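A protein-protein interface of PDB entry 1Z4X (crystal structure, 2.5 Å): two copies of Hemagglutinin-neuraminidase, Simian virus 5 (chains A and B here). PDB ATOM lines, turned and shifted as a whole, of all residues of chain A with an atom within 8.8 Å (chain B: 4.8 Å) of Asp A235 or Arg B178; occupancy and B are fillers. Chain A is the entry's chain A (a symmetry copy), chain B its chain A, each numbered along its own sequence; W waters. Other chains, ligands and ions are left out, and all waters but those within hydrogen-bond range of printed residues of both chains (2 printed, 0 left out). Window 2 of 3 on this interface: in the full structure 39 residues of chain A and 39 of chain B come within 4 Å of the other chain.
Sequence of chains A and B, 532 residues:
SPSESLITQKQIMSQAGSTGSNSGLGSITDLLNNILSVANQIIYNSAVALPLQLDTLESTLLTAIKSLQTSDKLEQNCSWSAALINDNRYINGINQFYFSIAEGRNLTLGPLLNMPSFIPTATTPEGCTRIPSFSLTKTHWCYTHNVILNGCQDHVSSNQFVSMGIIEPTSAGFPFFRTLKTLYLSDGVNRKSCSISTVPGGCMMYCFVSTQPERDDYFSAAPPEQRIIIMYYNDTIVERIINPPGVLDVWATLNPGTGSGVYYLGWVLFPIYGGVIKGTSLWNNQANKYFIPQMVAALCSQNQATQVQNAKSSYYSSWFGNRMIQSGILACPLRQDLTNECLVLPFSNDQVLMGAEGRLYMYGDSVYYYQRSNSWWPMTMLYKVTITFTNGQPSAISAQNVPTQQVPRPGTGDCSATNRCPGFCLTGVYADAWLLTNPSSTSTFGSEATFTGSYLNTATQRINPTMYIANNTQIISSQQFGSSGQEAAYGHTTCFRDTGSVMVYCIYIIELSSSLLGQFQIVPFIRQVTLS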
ATOM      1  N   PHE A 161     -13.850  30.927  -9.830  1.00  0.00           N
ATOM      2  CA  PHE A 161     -14.638  30.078 -10.726  1.00  0.00           C
ATOM      3  C   PHE A 161     -15.647  30.916 -11.508  1.00  0.00           C
ATOM      4  O   PHE A 161     -16.372  31.716 -10.921  1.00  0.00           O
ATOM      5  CB  PHE A 161     -15.392  29.008  -9.921  1.00  0.00           C
ATOM      6  CG  PHE A 161     -16.337  28.162 -10.747  1.00  0.00           C
ATOM      7  CD1 PHE A 161     -15.887  27.009 -11.393  1.00  0.00           C
ATOM      8  CD2 PHE A 161     -17.672  28.534 -10.899  1.00  0.00           C
ATOM      9  CE1 PHE A 161     -16.757  26.242 -12.180  1.00  0.00           C
ATOM     10  CE2 PHE A 161     -18.547  27.776 -11.682  1.00  0.00           C
ATOM     11  CZ  PHE A 161     -18.086  26.629 -12.322  1.00  0.00           C
ATOM     12  N   VAL A 162     -15.692  30.736 -12.826  1.00  0.00           N
ATOM     13  CA  VAL A 162     -16.637  31.470 -13.664  1.00  0.00           C
ATOM     14  C   VAL A 162     -17.460  30.455 -14.432  1.00  0.00           C
ATOM     15  O   VAL A 162     -16.958  29.409 -14.824  1.00  0.00           O
ATOM     16  CB  VAL A 162     -15.934  32.414 -14.668  1.00  0.00           C
ATOM     17  CG1 VAL A 162     -16.971  33.098 -15.558  1.00  0.00           C
ATOM     18  CG2 VAL A 162     -15.116  33.453 -13.919  1.00  0.00           C
ATOM     19  N   MET A 164     -21.087  30.184 -17.261  1.00  0.00           N
ATOM     20  CA  MET A 164     -22.061  30.908 -18.069  1.00  0.00           C
ATOM     21  C   MET A 164     -22.963  29.917 -18.775  1.00  0.00           C
ATOM     22  O   MET A 164     -22.562  28.787 -19.062  1.00  0.00           O
ATOM     23  CB  MET A 164     -21.371  31.837 -19.081  1.00  0.00           C
ATOM     24  CG  MET A 164     -20.580  31.161 -20.186  1.00  0.00           C
ATOM     25  SD  MET A 164     -19.780  32.414 -21.244  1.00  0.00           S
ATOM     26  CE  MET A 164     -18.401  32.878 -20.222  1.00  0.00           C
ATOM     27  N   THR A 179     -25.522  25.100 -17.879  1.00  0.00           N
ATOM     28  CA  THR A 179     -24.167  25.620 -18.013  1.00  0.00           C
ATOM     29  C   THR A 179     -23.623  25.235 -19.378  1.00  0.00           C
ATOM     30  O   THR A 179     -23.624  24.056 -19.733  1.00  0.00           O
ATOM     31  CB  THR A 179     -23.218  25.016 -16.956  1.00  0.00           C
ATOM     32  OG1 THR A 179     -23.678  25.351 -15.643  1.00  0.00           O
ATOM     33  CG2 THR A 179     -21.803  25.543 -17.146  1.00  0.00           C
ATOM     34  N   LEU A 180     -23.148  26.219 -20.138  1.00  0.00           N
ATOM     35  CA  LEU A 180     -22.592  25.954 -21.463  1.00  0.00           C
ATOM     36  C   LEU A 180     -21.077  26.158 -21.519  1.00  0.00           C
ATOM     37  O   LEU A 180     -20.433  25.839 -22.519  1.00  0.00           O
ATOM     38  CB  LEU A 180     -23.268  26.833 -22.509  1.00  0.00           C
ATOM     39  CG  LEU A 180     -24.746  26.530 -22.747  1.00  0.00           C
ATOM     40  CD1 LEU A 180     -25.240  27.363 -23.919  1.00  0.00           C
ATOM     41  CD2 LEU A 180     -24.933  25.051 -23.022  1.00  0.00           C
ATOM     42  N   LYS A 181     -20.516  26.698 -20.444  1.00  0.00           N
ATOM     43  CA  LYS A 181     -19.079  26.922 -20.367  1.00  0.00           C
ATOM     44  C   LYS A 181     -18.677  27.192 -18.932  1.00  0.00           C
ATOM     45  O   LYS A 181     -19.383  27.858 -18.182  1.00  0.00           O
ATOM     46  CB  LYS A 181     -18.631  28.105 -21.232  1.00  0.00           C
ATOM     47  CG  LYS A 181     -17.107  28.227 -21.304  1.00  0.00           C
ATOM     48  CD  LYS A 181     -16.636  29.563 -21.879  1.00  0.00           C
ATOM     49  CE  LYS A 181     -17.140  29.785 -23.292  1.00  0.00           C
ATOM     50  NZ  LYS A 181     -16.755  28.662 -24.193  1.00  0.00           N
ATOM     51  N   THR A 182     -17.519  26.672 -18.571  1.00  0.00           N
ATOM     52  CA  THR A 182     -16.974  26.806 -17.239  1.00  0.00           C
ATOM     53  C   THR A 182     -15.530  27.302 -17.384  1.00  0.00           C
ATOM     54  O   THR A 182     -14.865  27.004 -18.373  1.00  0.00           O
ATOM     55  CB  THR A 182     -17.049  25.420 -16.553  1.00  0.00           C
ATOM     56  OG1 THR A 182     -18.141  25.406 -15.622  1.00  0.00           O
ATOM     57  CG2 THR A 182     -15.774  25.065 -15.877  1.00  0.00           C
ATOM     58  N   LEU A 183     -15.065  28.088 -16.418  1.00  0.00           N
ATOM     59  CA  LEU A 183     -13.694  28.602 -16.424  1.00  0.00           C
ATOM     60  C   LEU A 183     -13.206  28.663 -14.996  1.00  0.00           C
ATOM     61  O   LEU A 183     -13.979  28.945 -14.084  1.00  0.00           O
ATOM     62  CB  LEU A 183     -13.608  30.022 -16.995  1.00  0.00           C
ATOM     63  CG  LEU A 183     -14.043  30.324 -18.424  1.00  0.00           C
ATOM     64  CD1 LEU A 183     -15.516  30.714 -18.435  1.00  0.00           C
ATOM     65  CD2 LEU A 183     -13.212  31.469 -18.964  1.00  0.00           C
ATOM     66  N   TYR A 184     -11.923  28.406 -14.798  1.00  0.00           N
ATOM     67  CA  TYR A 184     -11.354  28.457 -13.460  1.00  0.00           C
ATOM     68  C   TYR A 184     -10.068  29.257 -13.552  1.00  0.00           C
ATOM     69  O   TYR A 184      -9.041  28.750 -14.012  1.00  0.00           O
ATOM     70  CB  TYR A 184     -11.082  27.041 -12.945  1.00  0.00           C
ATOM     71  CG  TYR A 184     -10.788  26.934 -11.457  1.00  0.00           C
ATOM     72  CD1 TYR A 184     -11.556  27.631 -10.514  1.00  0.00           C
ATOM     73  CD2 TYR A 184      -9.789  26.080 -10.987  1.00  0.00           C
ATOM     74  CE1 TYR A 184     -11.339  27.472  -9.143  1.00  0.00           C
ATOM     75  CE2 TYR A 184      -9.559  25.910  -9.619  1.00  0.00           C
ATOM     76  CZ  TYR A 184     -10.338  26.606  -8.701  1.00  0.00           C
ATOM     77  OH  TYR A 184     -10.121  26.415  -7.350  1.00  0.00           O
ATOM     78  N   LEU A 185     -10.141  30.518 -13.143  1.00  0.00           N
ATOM     79  CA  LEU A 185      -8.987  31.396 -13.170  1.00  0.00           C
ATOM     80  C   LEU A 185      -8.094  31.018 -11.990  1.00  0.00           C
ATOM     81  O   LEU A 185      -8.356  31.385 -10.838  1.00  0.00           O
ATOM     82  CB  LEU A 185      -9.443  32.855 -13.074  1.00  0.00           C
ATOM     83  CG  LEU A 185     -10.494  33.251 -14.124  1.00  0.00           C
ATOM     84  CD1 LEU A 185     -10.856  34.729 -13.980  1.00  0.00           C
ATOM     85  CD2 LEU A 185      -9.946  32.975 -15.521  1.00  0.00           C
ATOM     86  N   GLY A 201     -22.413  38.330 -26.091  1.00  0.00           N
ATOM     87  CA  GLY A 201     -21.451  37.288 -26.402  1.00  0.00           C
ATOM     88  C   GLY A 201     -20.578  36.760 -25.275  1.00  0.00           C
ATOM     89  O   GLY A 201     -19.646  35.988 -25.526  1.00  0.00           O
ATOM     90  N   GLY A 202     -20.854  37.148 -24.037  1.00  0.00           N
ATOM     91  CA  GLY A 202     -20.031  36.657 -22.946  1.00  0.00           C
ATOM     92  C   GLY A 202     -20.279  37.280 -21.584  1.00  0.00           C
ATOM     93  O   GLY A 202     -21.405  37.625 -21.238  1.00  0.00           O
ATOM     94  N   ILE A 230     -12.685  39.936 -19.724  1.00  0.00           N
ATOM     95  CA  ILE A 230     -13.804  39.678 -20.622  1.00  0.00           C
ATOM     96  C   ILE A 230     -13.654  38.238 -21.095  1.00  0.00           C
ATOM     97  O   ILE A 230     -12.593  37.838 -21.590  1.00  0.00           O
ATOM     98  CB  ILE A 230     -13.805  40.616 -21.854  1.00  0.00           C
ATOM     99  CG1 ILE A 230     -13.832  42.079 -21.400  1.00  0.00           C
ATOM    100  CG2 ILE A 230     -15.040  40.344 -22.712  1.00  0.00           C
ATOM    101  CD1 ILE A 230     -13.704  43.079 -22.535  1.00  0.00           C
ATOM    102  N   MET A 231     -14.713  37.458 -20.920  1.00  0.00           N
ATOM    103  CA  MET A 231     -14.705  36.059 -21.309  1.00  0.00           C
ATOM    104  C   MET A 231     -15.837  35.826 -22.299  1.00  0.00           C
ATOM    105  O   MET A 231     -17.013  35.828 -21.925  1.00  0.00           O
ATOM    106  CB  MET A 231     -14.880  35.184 -20.063  1.00  0.00           C
ATOM    107  CG  MET A 231     -13.768  35.391 -19.028  1.00  0.00           C
ATOM    108  SD  MET A 231     -14.186  34.880 -17.327  1.00  0.00           S
ATOM    109  CE  MET A 231     -15.153  36.312 -16.793  1.00  0.00           C
ATOM    110  N   TYR A 232     -15.477  35.643 -23.565  1.00  0.00           N
ATOM    111  CA  TYR A 232     -16.464  35.428 -24.608  1.00  0.00           C
ATOM    112  C   TYR A 232     -16.875  33.975 -24.687  1.00  0.00           C
ATOM    113  O   TYR A 232     -16.102  33.076 -24.357  1.00  0.00           O
ATOM    114  CB  TYR A 232     -15.907  35.881 -25.957  1.00  0.00           C
ATOM    115  CG  TYR A 232     -15.734  37.374 -26.014  1.00  0.00           C
ATOM    116  CD1 TYR A 232     -16.841  38.210 -26.114  1.00  0.00           C
ATOM    117  CD2 TYR A 232     -14.470  37.956 -25.922  1.00  0.00           C
ATOM    118  CE1 TYR A 232     -16.694  39.599 -26.127  1.00  0.00           C
ATOM    119  CE2 TYR A 232     -14.308  39.343 -25.931  1.00  0.00           C
ATOM    120  CZ  TYR A 232     -15.421  40.160 -26.032  1.00  0.00           C
ATOM    121  OH  TYR A 232     -15.269  41.538 -26.061  1.00  0.00           O
ATOM    122  N   TYR A 233     -18.104  33.755 -25.129  1.00  0.00           N
ATOM    123  CA  TYR A 233     -18.644  32.413 -25.254  1.00  0.00           C
ATOM    124  C   TYR A 233     -17.844  31.576 -26.245  1.00  0.00           C
ATOM    125  O   TYR A 233     -17.935  30.351 -26.256  1.00  0.00           O
ATOM    126  CB  TYR A 233     -20.103  32.494 -25.704  1.00  0.00           C
ATOM    127  CG  TYR A 233     -20.761  31.150 -25.853  1.00  0.00           C
ATOM    128  CD1 TYR A 233     -21.025  30.344 -24.736  1.00  0.00           C
ATOM    129  CD2 TYR A 233     -21.125  30.674 -27.113  1.00  0.00           C
ATOM    130  CE1 TYR A 233     -21.634  29.107 -24.880  1.00  0.00           C
ATOM    131  CE2 TYR A 233     -21.734  29.435 -27.265  1.00  0.00           C
ATOM    132  CZ  TYR A 233     -21.984  28.663 -26.151  1.00  0.00           C
ATOM    133  OH  TYR A 233     -22.593  27.449 -26.319  1.00  0.00           O
ATOM    134  N   ASN A 234     -17.073  32.258 -27.095  1.00  0.00           N
ATOM    135  CA  ASN A 234     -16.227  31.584 -28.086  1.00  0.00           C
ATOM    136  C   ASN A 234     -14.851  31.252 -27.517  1.00  0.00           C
ATOM    137  O   ASN A 234     -13.919  30.977 -28.261  1.00  0.00           O
ATOM    138  CB  ASN A 234     -16.048  32.425 -29.367  1.00  0.00           C
ATOM    139  CG  ASN A 234     -15.258  33.706 -29.141  1.00  0.00           C
ATOM    140  OD1 ASN A 234     -14.557  33.854 -28.137  1.00  0.00           O
ATOM    141  ND2 ASN A 234     -15.372  34.634 -30.093  1.00  0.00           N
ATOM    142  N   ASP A 235     -14.758  31.255 -26.188  1.00  0.00           N
ATOM    143  CA  ASP A 235     -13.542  30.936 -25.456  1.00  0.00           C
ATOM    144  C   ASP A 235     -12.354  31.889 -25.515  1.00  0.00           C
ATOM    145  O   ASP A 235     -11.277  31.560 -25.028  1.00  0.00           O
ATOM    146  CB  ASP A 235     -13.086  29.511 -25.784  1.00  0.00           C
ATOM    147  CG  ASP A 235     -13.040  28.626 -24.542  1.00  0.00           C
ATOM    148  OD1 ASP A 235     -14.071  28.544 -23.845  1.00  0.00           O
ATOM    149  OD2 ASP A 235     -11.980  28.024 -24.250  1.00  0.00           O
ATOM    150  N   THR A 236     -12.534  33.065 -26.103  1.00  0.00           N
ATOM    151  CA  THR A 236     -11.459  34.043 -26.127  1.00  0.00           C
ATOM    152  C   THR A 236     -11.514  34.725 -24.764  1.00  0.00           C
ATOM    153  O   THR A 236     -12.600  35.003 -24.259  1.00  0.00           O
ATOM    154  CB  THR A 236     -11.690  35.111 -27.204  1.00  0.00           C
ATOM    155  OG1 THR A 236     -11.393  34.557 -28.488  1.00  0.00           O
ATOM    156  CG2 THR A 236     -10.813  36.322 -26.970  1.00  0.00           C
ATOM    157  N   ILE A 237     -10.358  34.980 -24.163  1.00  0.00           N
ATOM    158  CA  ILE A 237     -10.295  35.638 -22.866  1.00  0.00           C
ATOM    159  C   ILE A 237      -9.309  36.792 -22.931  1.00  0.00           C
ATOM    160  O   ILE A 237      -8.167  36.626 -23.363  1.00  0.00           O
ATOM    161  CB  ILE A 237      -9.836  34.681 -21.755  1.00  0.00           C
ATOM    162  CG1 ILE A 237     -10.795  33.499 -21.663  1.00  0.00           C
ATOM    163  CG2 ILE A 237      -9.781  35.414 -20.421  1.00  0.00           C
ATOM    164  CD1 ILE A 237     -10.408  32.498 -20.601  1.00  0.00           C
ATOM    165  N   VAL A 238      -9.760  37.962 -22.496  1.00  0.00           N
ATOM    166  CA  VAL A 238      -8.931  39.155 -22.510  1.00  0.00           C
ATOM    167  C   VAL A 238      -8.978  39.808 -21.139  1.00  0.00           C
ATOM    168  O   VAL A 238     -10.032  40.271 -20.707  1.00  0.00           O
ATOM    169  CB  VAL A 238      -9.436  40.184 -23.550  1.00  0.00           C
ATOM    170  CG1 VAL A 238      -8.496  41.378 -23.605  1.00  0.00           C
ATOM    171  CG2 VAL A 238      -9.549  39.534 -24.917  1.00  0.00           C
ATOM    172  N   TRP B 141     -13.984  13.754 -20.766  1.00  0.00           N
ATOM    173  CA  TRP B 141     -14.774  12.938 -19.845  1.00  0.00           C
ATOM    174  C   TRP B 141     -16.273  13.176 -20.004  1.00  0.00           C
ATOM    175  O   TRP B 141     -16.701  14.227 -20.468  1.00  0.00           O
ATOM    176  CB  TRP B 141     -14.380  13.217 -18.391  1.00  0.00           C
ATOM    177  CG  TRP B 141     -14.465  14.672 -17.963  1.00  0.00           C
ATOM    178  CD1 TRP B 141     -13.431  15.555 -17.877  1.00  0.00           C
ATOM    179  CD2 TRP B 141     -15.640  15.388 -17.538  1.00  0.00           C
ATOM    180  NE1 TRP B 141     -13.882  16.769 -17.423  1.00  0.00           N
ATOM    181  CE2 TRP B 141     -15.231  16.696 -17.206  1.00  0.00           C
ATOM    182  CE3 TRP B 141     -16.991  15.048 -17.403  1.00  0.00           C
ATOM    183  CZ2 TRP B 141     -16.128  17.673 -16.748  1.00  0.00           C
ATOM    184  CZ3 TRP B 141     -17.890  16.021 -16.946  1.00  0.00           C
ATOM    185  CH2 TRP B 141     -17.451  17.317 -16.624  1.00  0.00           C
ATOM    186  N   MET B 164     -20.194  17.012 -19.737  1.00  0.00           N
ATOM    187  CA  MET B 164     -18.981  16.585 -20.424  1.00  0.00           C
ATOM    188  C   MET B 164     -17.969  17.712 -20.402  1.00  0.00           C
ATOM    189  O   MET B 164     -18.333  18.889 -20.353  1.00  0.00           O
ATOM    190  CB  MET B 164     -19.278  16.144 -21.866  1.00  0.00           C
ATOM    191  CG  MET B 164     -19.739  17.230 -22.821  1.00  0.00           C
ATOM    192  SD  MET B 164     -20.109  16.512 -24.458  1.00  0.00           S
ATOM    193  CE  MET B 164     -21.700  15.784 -24.148  1.00  0.00           C
ATOM    194  N   GLY B 165     -16.693  17.351 -20.414  1.00  0.00           N
ATOM    195  CA  GLY B 165     -15.660  18.361 -20.385  1.00  0.00           C
ATOM    196  C   GLY B 165     -14.262  17.785 -20.482  1.00  0.00           C
ATOM    197  O   GLY B 165     -14.060  16.661 -20.947  1.00  0.00           O
ATOM    198  N   ILE B 166     -13.298  18.567 -20.013  1.00  0.00           N
ATOM    199  CA  ILE B 166     -11.902  18.176 -20.066  1.00  0.00           C
ATOM    200  C   ILE B 166     -11.214  18.374 -18.719  1.00  0.00           C
ATOM    201  O   ILE B 166     -11.802  18.912 -17.782  1.00  0.00           O
ATOM    202  CB  ILE B 166     -11.169  19.025 -21.106  1.00  0.00           C
ATOM    203  CG1 ILE B 166     -11.145  20.482 -20.628  1.00  0.00           C
ATOM    204  CG2 ILE B 166     -11.875  18.913 -22.459  1.00  0.00           C
ATOM    205  CD1 ILE B 166     -10.451  21.439 -21.560  1.00  0.00           C
ATOM    206  N   GLU B 168      -7.800  19.991 -16.772  1.00  0.00           N
ATOM    207  CA  GLU B 168      -6.710  20.941 -16.923  1.00  0.00           C
ATOM    208  C   GLU B 168      -6.096  21.213 -15.560  1.00  0.00           C
ATOM    209  O   GLU B 168      -6.779  21.170 -14.541  1.00  0.00           O
ATOM    210  CB  GLU B 168      -7.199  22.249 -17.549  1.00  0.00           C
ATOM    211  CG  GLU B 168      -8.192  23.029 -16.710  1.00  0.00           C
ATOM    212  CD  GLU B 168      -8.581  24.347 -17.362  1.00  0.00           C
ATOM    213  OE1 GLU B 168      -8.637  24.395 -18.612  1.00  0.00           O
ATOM    214  OE2 GLU B 168      -8.843  25.331 -16.630  1.00  0.00           O
ATOM    215  N   PHE B 176      -8.526  20.050 -12.472  1.00  0.00           N
ATOM    216  CA  PHE B 176      -9.768  20.780 -12.406  1.00  0.00           C
ATOM    217  C   PHE B 176     -10.567  20.201 -13.558  1.00  0.00           C
ATOM    218  O   PHE B 176     -10.143  20.284 -14.707  1.00  0.00           O
ATOM    219  CB  PHE B 176      -9.568  22.277 -12.643  1.00  0.00           C
ATOM    220  CG  PHE B 176     -10.824  22.989 -13.099  1.00  0.00           C
ATOM    221  CD1 PHE B 176     -12.019  22.845 -12.393  1.00  0.00           C
ATOM    222  CD2 PHE B 176     -10.811  23.801 -14.230  1.00  0.00           C
ATOM    223  CE1 PHE B 176     -13.183  23.498 -12.802  1.00  0.00           C
ATOM    224  CE2 PHE B 176     -11.970  24.463 -14.651  1.00  0.00           C
ATOM    225  CZ  PHE B 176     -13.157  24.309 -13.936  1.00  0.00           C
ATOM    226  N   PHE B 177     -11.702  19.586 -13.260  1.00  0.00           N
ATOM    227  CA  PHE B 177     -12.542  19.036 -14.308  1.00  0.00           C
ATOM    228  C   PHE B 177     -13.405  20.162 -14.842  1.00  0.00           C
ATOM    229  O   PHE B 177     -14.381  20.573 -14.215  1.00  0.00           O
ATOM    230  CB  PHE B 177     -13.391  17.891 -13.769  1.00  0.00           C
ATOM    231  CG  PHE B 177     -12.608  16.634 -13.548  1.00  0.00           C
ATOM    232  CD1 PHE B 177     -11.583  16.599 -12.607  1.00  0.00           C
ATOM    233  CD2 PHE B 177     -12.847  15.512 -14.315  1.00  0.00           C
ATOM    234  CE1 PHE B 177     -10.805  15.458 -12.442  1.00  0.00           C
ATOM    235  CE2 PHE B 177     -12.073  14.363 -14.157  1.00  0.00           C
ATOM    236  CZ  PHE B 177     -11.048  14.341 -13.215  1.00  0.00           C
ATOM    237  N   ARG B 178     -13.011  20.670 -16.003  1.00  0.00           N
ATOM    238  CA  ARG B 178     -13.698  21.771 -16.643  1.00  0.00           C
ATOM    239  C   ARG B 178     -14.890  21.310 -17.482  1.00  0.00           C
ATOM    240  O   ARG B 178     -14.724  20.634 -18.495  1.00  0.00           O
ATOM    241  CB  ARG B 178     -12.711  22.532 -17.530  1.00  0.00           C
ATOM    242  CG  ARG B 178     -13.258  23.833 -18.052  1.00  0.00           C
ATOM    243  CD  ARG B 178     -12.387  24.443 -19.111  1.00  0.00           C
ATOM    244  NE  ARG B 178     -12.969  25.700 -19.562  1.00  0.00           N
ATOM    245  CZ  ARG B 178     -12.592  26.361 -20.647  1.00  0.00           C
ATOM    246  NH1 ARG B 178     -11.619  25.887 -21.411  1.00  0.00           N
ATOM    247  NH2 ARG B 178     -13.194  27.497 -20.973  1.00  0.00           N
ATOM    248  N   THR B 179     -16.090  21.685 -17.049  1.00  0.00           N
ATOM    249  CA  THR B 179     -17.309  21.334 -17.768  1.00  0.00           C
ATOM    250  C   THR B 179     -17.440  22.232 -18.986  1.00  0.00           C
ATOM    251  O   THR B 179     -17.402  23.456 -18.857  1.00  0.00           O
ATOM    252  CB  THR B 179     -18.566  21.555 -16.899  1.00  0.00           C
ATOM    253  OG1 THR B 179     -18.502  20.728 -15.734  1.00  0.00           O
ATOM    254  CG2 THR B 179     -19.824  21.222 -17.688  1.00  0.00           C
ATOM    255  N   LEU B 180     -17.605  21.634 -20.163  1.00  0.00           N
ATOM    256  CA  LEU B 180     -17.751  22.407 -21.394  1.00  0.00           C
ATOM    257  C   LEU B 180     -19.165  22.329 -21.974  1.00  0.00           C
ATOM    258  O   LEU B 180     -19.497  23.036 -22.927  1.00  0.00           O
ATOM    259  CB  LEU B 180     -16.742  21.943 -22.437  1.00  0.00           C
ATOM    260  CG  LEU B 180     -15.281  22.224 -22.088  1.00  0.00           C
ATOM    261  CD1 LEU B 180     -14.408  21.861 -23.280  1.00  0.00           C
ATOM    262  CD2 LEU B 180     -15.108  23.685 -21.722  1.00  0.00           C
HETATM  263  O   HOH W   1      -7.425  26.574 -14.669  1.00  0.00           O
HETATM  264  O   HOH W   2     -10.286  27.532 -17.362  1.00  0.00           O
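The guanidinium group (NH2) of Arg B178 lies within salt-bridge range of the side-chain carboxylate (OD1) of Asp A235 (3.2 Å). O of Leu B180 lies close to O of Leu A180, at 3.0 Å. The backbone carbonyl oxygen of Thr B179 lies close to the backbone NH of Thr A182. The guanidinium group of Arg B178 sits at hydrogen-bond distance from the backbone carbonyl oxygen of Thr A182 (2.6 Å).
Water W1 lies within hydrogen-bond range of the side-chain carboxylate of Glu B168 and the backbone carbonyl oxygen of Tyr A184. Water W2 lies within hydrogen-bond range of the side-chain carboxylate (OE2) of Glu B168 and the backbone NH (N) of Tyr A184.
Thr A179 touches none of the printed residues of chain B. Printed residues of chain B within 4 Å of Leu A180: Leu B180 (3.0 Å). Printed residues of chain B within 4 Å of Tyr A184: Phe B176 (3.2 Å). Of the printed residues of chain B, Asp A235 touches Arg B178 (3.2 Å). No residue of chain A comes within 4 Å of Gly B165. Of the printed residues of chain A, Phe B176 touches Thr A182 (3.3 Å) and Tyr A184 (3.2 Å). Of the printed residues of chain A, Arg B178 touches Lys A181 (3.99 Å), Thr A182 (2.6 Å), Leu A183 (3.9 Å) and Asp A235 (3.2 Å). Printed residues of chain A within 4 Å of Leu B180: Leu A180 (3.0 Å). The nearest printed residue of chain B that does not touch Asp A235 is Leu B180 (5.4 Å).
Leu A180 touches its own counterpart, Leu B180. 3 positions are printed for both chains.
O of Ile B166 sits at hydrogen-bond distance from N of Arg B178. N of Val A162 is in hydrogen-bond range of O of Leu A183 (2.8 Å). The backbone carbonyl oxygen (O) of Glu B168 sits at hydrogen-bond distance from the backbone NH (N) of Phe B176. The backbone carbonyl oxygen (O) of Met B164 is in hydrogen-bond range of the backbone NH (N) of Leu B180 (2.8 Å). O of Lys A181 lies within hydrogen-bond range of N of Met A164. The side-chain amino group (NZ) of Lys A181 is in salt-bridge range of the side-chain carboxylate (OD1) of Asp A235, at 2.7 Å.
Among the printed residues, merely in contact across the chains: Tyr A184 with Phe B176 (3.2 Å), Thr A182 with Phe B176 (3.3 Å), Leu A183 with Arg B178 (3.9 Å), Lys A181 with Thr B179 (3.9 Å) and Lys A181 with Arg B178 (3.99 Å).
Of the 21 printed residues of chain A, 6 touch a printed residue of chain B. Hydrophobic or aromatic side chains of chain A within 4 Å of the printed part of chain B: Leu A183 and Tyr A184. Among the printed residues, Asp or Glu carboxylates within 4 Å of a Lys or Arg side-chain nitrogen of the other chain: Asp A235 with Arg B178.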
